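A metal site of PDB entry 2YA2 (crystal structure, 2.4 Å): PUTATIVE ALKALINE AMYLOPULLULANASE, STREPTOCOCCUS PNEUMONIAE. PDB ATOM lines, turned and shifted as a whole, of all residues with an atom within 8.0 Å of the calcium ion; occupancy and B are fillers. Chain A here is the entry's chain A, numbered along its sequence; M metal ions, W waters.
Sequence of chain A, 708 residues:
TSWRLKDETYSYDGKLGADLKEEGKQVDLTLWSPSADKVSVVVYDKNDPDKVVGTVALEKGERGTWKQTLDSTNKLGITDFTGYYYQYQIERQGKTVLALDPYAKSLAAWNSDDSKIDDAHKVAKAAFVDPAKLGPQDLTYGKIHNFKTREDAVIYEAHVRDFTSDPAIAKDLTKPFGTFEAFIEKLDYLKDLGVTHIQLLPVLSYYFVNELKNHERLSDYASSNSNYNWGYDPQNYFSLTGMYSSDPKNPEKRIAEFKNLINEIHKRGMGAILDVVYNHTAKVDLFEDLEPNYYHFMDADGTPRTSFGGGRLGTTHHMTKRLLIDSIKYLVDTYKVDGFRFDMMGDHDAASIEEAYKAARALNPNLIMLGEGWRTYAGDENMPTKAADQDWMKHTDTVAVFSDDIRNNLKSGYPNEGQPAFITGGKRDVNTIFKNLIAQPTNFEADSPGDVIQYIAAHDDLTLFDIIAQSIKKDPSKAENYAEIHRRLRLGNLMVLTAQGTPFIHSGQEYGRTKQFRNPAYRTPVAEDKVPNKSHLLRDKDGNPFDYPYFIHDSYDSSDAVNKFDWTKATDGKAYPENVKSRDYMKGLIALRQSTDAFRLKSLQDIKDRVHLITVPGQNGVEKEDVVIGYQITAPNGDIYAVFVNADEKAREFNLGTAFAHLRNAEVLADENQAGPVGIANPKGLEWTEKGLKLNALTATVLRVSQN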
ATOM      1  N   ARG A 150     -10.034  11.886  24.731  1.00  0.00           N
ATOM      2  CA  ARG A 150      -9.943  13.258  25.293  1.00  0.00           C
ATOM      3  C   ARG A 150      -9.997  14.415  24.264  1.00  0.00           C
ATOM      4  O   ARG A 150     -10.695  15.411  24.491  1.00  0.00           O
ATOM      5  CB  ARG A 150      -8.702  13.448  26.217  1.00  0.00           C
ATOM      6  CG  ARG A 150      -7.569  12.417  26.021  1.00  0.00           C
ATOM      7  CD  ARG A 150      -6.197  13.051  25.890  1.00  0.00           C
ATOM      8  NE  ARG A 150      -5.442  13.052  27.153  1.00  0.00           N
ATOM      9  CZ  ARG A 150      -4.116  13.157  27.272  1.00  0.00           C
ATOM     10  NH1 ARG A 150      -3.338  13.254  26.220  1.00  0.00           N
ATOM     11  NH2 ARG A 150      -3.579  13.163  28.467  1.00  0.00           N
ATOM     12  N   GLN A 390       2.178  21.262  34.776  1.00  0.00           N
ATOM     13  CA  GLN A 390       2.446  21.380  33.350  1.00  0.00           C
ATOM     14  C   GLN A 390       3.721  20.648  32.866  1.00  0.00           C
ATOM     15  O   GLN A 390       3.700  20.013  31.788  1.00  0.00           O
ATOM     16  CB  GLN A 390       2.496  22.861  32.947  1.00  0.00           C
ATOM     17  CG  GLN A 390       1.107  23.538  32.935  1.00  0.00           C
ATOM     18  CD  GLN A 390       1.161  25.017  32.596  1.00  0.00           C
ATOM     19  OE1 GLN A 390       2.106  25.710  32.942  1.00  0.00           O
ATOM     20  NE2 GLN A 390       0.113  25.511  31.944  1.00  0.00           N
ATOM     21  N   TRP A 392       4.895  18.023  33.885  1.00  0.00           N
ATOM     22  CA  TRP A 392       4.613  16.579  33.916  1.00  0.00           C
ATOM     23  C   TRP A 392       4.043  16.088  32.589  1.00  0.00           C
ATOM     24  O   TRP A 392       4.078  14.897  32.325  1.00  0.00           O
ATOM     25  CB  TRP A 392       3.643  16.251  35.073  1.00  0.00           C
ATOM     26  CG  TRP A 392       3.209  14.810  35.259  1.00  0.00           C
ATOM     27  CD1 TRP A 392       3.995  13.678  35.220  1.00  0.00           C
ATOM     28  CD2 TRP A 392       1.871  14.345  35.566  1.00  0.00           C
ATOM     29  NE1 TRP A 392       3.224  12.535  35.452  1.00  0.00           N
ATOM     30  CE2 TRP A 392       1.926  12.927  35.663  1.00  0.00           C
ATOM     31  CE3 TRP A 392       0.632  15.000  35.732  1.00  0.00           C
ATOM     32  CZ2 TRP A 392       0.790  12.156  35.922  1.00  0.00           C
ATOM     33  CZ3 TRP A 392      -0.501  14.240  35.997  1.00  0.00           C
ATOM     34  CH2 TRP A 392      -0.417  12.817  36.092  1.00  0.00           C
ATOM     35  N   MET A 393       3.511  16.985  31.751  1.00  0.00           N
ATOM     36  CA  MET A 393       2.844  16.547  30.504  1.00  0.00           C
ATOM     37  C   MET A 393       3.731  15.703  29.566  1.00  0.00           C
ATOM     38  O   MET A 393       3.238  14.832  28.850  1.00  0.00           O
ATOM     39  CB  MET A 393       2.194  17.731  29.794  1.00  0.00           C
ATOM     40  CG  MET A 393       0.999  18.361  30.562  1.00  0.00           C
ATOM     41  SD  MET A 393      -0.348  17.200  30.955  1.00  0.00           S
ATOM     42  CE  MET A 393       0.038  16.455  32.543  1.00  0.00           C
ATOM     43  N   LYS A 394       5.047  15.943  29.604  1.00  0.00           N
ATOM     44  CA  LYS A 394       6.008  15.179  28.790  1.00  0.00           C
ATOM     45  C   LYS A 394       6.263  13.763  29.293  1.00  0.00           C
ATOM     46  O   LYS A 394       6.906  13.000  28.603  1.00  0.00           O
ATOM     47  CB  LYS A 394       7.348  15.923  28.619  1.00  0.00           C
ATOM     48  CG  LYS A 394       8.322  15.856  29.823  1.00  0.00           C
ATOM     49  CD  LYS A 394       9.293  17.060  29.821  1.00  0.00           C
ATOM     50  CE  LYS A 394       8.498  18.374  29.795  1.00  0.00           C
ATOM     51  NZ  LYS A 394       8.981  19.445  30.694  1.00  0.00           N
ATOM     52  N   HIS A 395       5.749  13.406  30.475  1.00  0.00           N
ATOM     53  CA  HIS A 395       5.952  12.042  30.980  1.00  0.00           C
ATOM     54  C   HIS A 395       4.639  11.249  31.078  1.00  0.00           C
ATOM     55  O   HIS A 395       4.622  10.147  31.646  1.00  0.00           O
ATOM     56  CB  HIS A 395       6.645  12.000  32.338  1.00  0.00           C
ATOM     57  CG  HIS A 395       7.843  12.909  32.471  1.00  0.00           C
ATOM     58  ND1 HIS A 395       9.116  12.540  32.119  1.00  0.00           N
ATOM     59  CD2 HIS A 395       7.957  14.144  33.019  1.00  0.00           C
ATOM     60  CE1 HIS A 395       9.958  13.515  32.393  1.00  0.00           C
ATOM     61  NE2 HIS A 395       9.280  14.513  32.932  1.00  0.00           N
ATOM     62  N   THR A 396       3.541  11.803  30.583  1.00  0.00           N
ATOM     63  CA  THR A 396       2.231  11.128  30.688  1.00  0.00           C
ATOM     64  C   THR A 396       1.245  11.564  29.594  1.00  0.00           C
ATOM     65  O   THR A 396       1.314  12.701  29.094  1.00  0.00           O
ATOM     66  CB  THR A 396       1.590  11.348  32.100  1.00  0.00           C
ATOM     67  OG1 THR A 396       0.584  10.358  32.347  1.00  0.00           O
ATOM     68  CG2 THR A 396       0.982  12.740  32.217  1.00  0.00           C
ATOM     69  N   ASP A 397       0.365  10.643  29.204  1.00  0.00           N
ATOM     70  CA  ASP A 397      -0.769  10.928  28.322  1.00  0.00           C
ATOM     71  C   ASP A 397      -2.019  10.412  29.044  1.00  0.00           C
ATOM     72  O   ASP A 397      -2.652   9.400  28.640  1.00  0.00           O
ATOM     73  CB  ASP A 397      -0.611  10.262  26.947  1.00  0.00           C
ATOM     74  CG  ASP A 397       0.426  10.944  26.064  1.00  0.00           C
ATOM     75  OD1 ASP A 397       0.681  12.149  26.203  1.00  0.00           O
ATOM     76  OD2 ASP A 397       0.981  10.258  25.203  1.00  0.00           O
ATOM     77  N   THR A 398      -2.356  11.091  30.132  1.00  0.00           N
ATOM     78  CA  THR A 398      -3.421  10.686  30.998  1.00  0.00           C
ATOM     79  C   THR A 398      -4.271  11.920  31.319  1.00  0.00           C
ATOM     80  O   THR A 398      -5.212  12.207  30.580  1.00  0.00           O
ATOM     81  CB  THR A 398      -2.870   9.908  32.249  1.00  0.00           C
ATOM     82  OG1 THR A 398      -1.947  10.724  32.992  1.00  0.00           O
ATOM     83  CG2 THR A 398      -2.150   8.627  31.812  1.00  0.00           C
ATOM     84  N   VAL A 399      -3.873  12.674  32.345  1.00  0.00           N
ATOM     85  CA  VAL A 399      -4.564  13.888  32.821  1.00  0.00           C
ATOM     86  C   VAL A 399      -4.052  15.120  32.099  1.00  0.00           C
ATOM     87  O   VAL A 399      -2.856  15.394  32.078  1.00  0.00           O
ATOM     88  CB  VAL A 399      -4.271  14.096  34.341  1.00  0.00           C
ATOM     89  CG1 VAL A 399      -4.938  15.360  34.883  1.00  0.00           C
ATOM     90  CG2 VAL A 399      -4.631  12.817  35.195  1.00  0.00           C
ATOM     91  N   PHE A 444       5.232  25.272  28.298  1.00  0.00           N
ATOM     92  CA  PHE A 444       5.503  23.880  28.655  1.00  0.00           C
ATOM     93  C   PHE A 444       5.436  22.953  27.439  1.00  0.00           C
ATOM     94  O   PHE A 444       4.825  23.301  26.410  1.00  0.00           O
ATOM     95  CB  PHE A 444       4.560  23.393  29.762  1.00  0.00           C
ATOM     96  CG  PHE A 444       3.159  23.065  29.309  1.00  0.00           C
ATOM     97  CD1 PHE A 444       2.815  21.764  28.894  1.00  0.00           C
ATOM     98  CD2 PHE A 444       2.157  24.039  29.338  1.00  0.00           C
ATOM     99  CE1 PHE A 444       1.513  21.449  28.499  1.00  0.00           C
ATOM    100  CE2 PHE A 444       0.845  23.722  28.966  1.00  0.00           C
ATOM    101  CZ  PHE A 444       0.512  22.425  28.537  1.00  0.00           C
ATOM    102  N   GLU A 445       6.061  21.781  27.549  1.00  0.00           N
ATOM    103  CA  GLU A 445       6.047  20.765  26.480  1.00  0.00           C
ATOM    104  C   GLU A 445       4.807  19.855  26.489  1.00  0.00           C
ATOM    105  O   GLU A 445       4.641  19.030  27.371  1.00  0.00           O
ATOM    106  CB  GLU A 445       7.323  19.916  26.527  1.00  0.00           C
ATOM    107  CG  GLU A 445       7.448  18.919  25.330  1.00  0.00           C
ATOM    108  CD  GLU A 445       8.663  18.001  25.426  1.00  0.00           C
ATOM    109  OE1 GLU A 445       9.739  18.442  25.885  1.00  0.00           O
ATOM    110  OE2 GLU A 445       8.529  16.827  25.020  1.00  0.00           O
ATOM    111  N   ALA A 446       3.959  20.027  25.480  1.00  0.00           N
ATOM    112  CA  ALA A 446       2.849  19.102  25.183  1.00  0.00           C
ATOM    113  C   ALA A 446       3.210  18.144  24.039  1.00  0.00           C
ATOM    114  O   ALA A 446       3.106  18.520  22.875  1.00  0.00           O
ATOM    115  CB  ALA A 446       1.623  19.899  24.809  1.00  0.00           C
ATOM    116  N   ASP A 447       3.624  16.921  24.369  1.00  0.00           N
ATOM    117  CA  ASP A 447       3.973  15.906  23.371  1.00  0.00           C
ATOM    118  C   ASP A 447       2.762  15.110  22.858  1.00  0.00           C
ATOM    119  O   ASP A 447       2.949  14.101  22.183  1.00  0.00           O
ATOM    120  CB  ASP A 447       4.985  14.933  23.972  1.00  0.00           C
ATOM    121  CG  ASP A 447       4.392  14.128  25.142  1.00  0.00           C
ATOM    122  OD1 ASP A 447       3.272  14.521  25.583  1.00  0.00           O
ATOM    123  OD2 ASP A 447       5.010  13.124  25.602  1.00  0.00           O
ATOM    124  N   SER A 448       1.541  15.534  23.207  1.00  0.00           N
ATOM    125  CA  SER A 448       0.278  15.025  22.603  1.00  0.00           C
ATOM    126  C   SER A 448      -0.761  16.131  22.754  1.00  0.00           C
ATOM    127  O   SER A 448      -0.774  16.760  23.796  1.00  0.00           O
ATOM    128  CB  SER A 448      -0.208  13.731  23.277  1.00  0.00           C
ATOM    129  OG  SER A 448      -1.617  13.527  23.103  1.00  0.00           O
ATOM    130  N   PRO A 449      -1.604  16.390  21.718  1.00  0.00           N
ATOM    131  CA  PRO A 449      -2.507  17.530  21.821  1.00  0.00           C
ATOM    132  C   PRO A 449      -3.576  17.352  22.891  1.00  0.00           C
ATOM    133  O   PRO A 449      -4.120  18.331  23.346  1.00  0.00           O
ATOM    134  CB  PRO A 449      -3.162  17.614  20.445  1.00  0.00           C
ATOM    135  CG  PRO A 449      -3.080  16.231  19.908  1.00  0.00           C
ATOM    136  CD  PRO A 449      -1.786  15.676  20.441  1.00  0.00           C
ATOM    137  N   GLY A 450      -3.843  16.120  23.288  1.00  0.00           N
ATOM    138  CA  GLY A 450      -4.743  15.850  24.397  1.00  0.00           C
ATOM    139  C   GLY A 450      -4.206  16.205  25.780  1.00  0.00           C
ATOM    140  O   GLY A 450      -4.964  16.134  26.759  1.00  0.00           O
ATOM    141  N   ASP A 451      -2.908  16.544  25.884  1.00  0.00           N
ATOM    142  CA  ASP A 451      -2.324  17.079  27.123  1.00  0.00           C
ATOM    143  C   ASP A 451      -2.842  18.499  27.440  1.00  0.00           C
ATOM    144  O   ASP A 451      -2.715  18.977  28.585  1.00  0.00           O
ATOM    145  CB  ASP A 451      -0.788  17.190  27.014  1.00  0.00           C
ATOM    146  CG  ASP A 451      -0.086  15.865  27.055  1.00  0.00           C
ATOM    147  OD1 ASP A 451      -0.628  14.864  27.552  1.00  0.00           O
ATOM    148  OD2 ASP A 451       1.092  15.822  26.606  1.00  0.00           O
ATOM    149  N   VAL A 452      -3.412  19.155  26.428  1.00  0.00           N
ATOM    150  CA  VAL A 452      -3.719  20.588  26.474  1.00  0.00           C
ATOM    151  C   VAL A 452      -5.214  20.833  26.617  1.00  0.00           C
ATOM    152  O   VAL A 452      -5.989  20.451  25.745  1.00  0.00           O
ATOM    153  CB  VAL A 452      -3.193  21.302  25.182  1.00  0.00           C
ATOM    154  CG1 VAL A 452      -3.542  22.750  25.185  1.00  0.00           C
ATOM    155  CG2 VAL A 452      -1.690  21.152  25.040  1.00  0.00           C
HETATM  156 CA    CA M   1       1.811  13.768  27.235  1.00  0.00          CA
HETATM  157  O   HOH W   1       3.457  12.197  27.454  1.00  0.00           O
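Water W1 bridges OD2 of Asp 447 (2.6 Å) and N of Thr 396 (3.2 Å).
The calcium ion is bound by O of Thr 396, OD1 of Asp 397, OD2 of Asp 451, water W1, OD1 of Asp 447, O of Met 393 and OD1 of Asp 451.
The guanidinium group (NH1) of Arg 150 lies close to the side-chain carboxylate (OD1) of Asp 451, 3.4 Å away.
The side-chain hydroxyl (OG1) of Thr 398 sits at hydrogen-bond distance from the side-chain hydroxyl (OG1) of Thr 396 (2.6 Å).
OD2 of Asp 451 lies close to N of Ser 448, 3.4 Å away.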
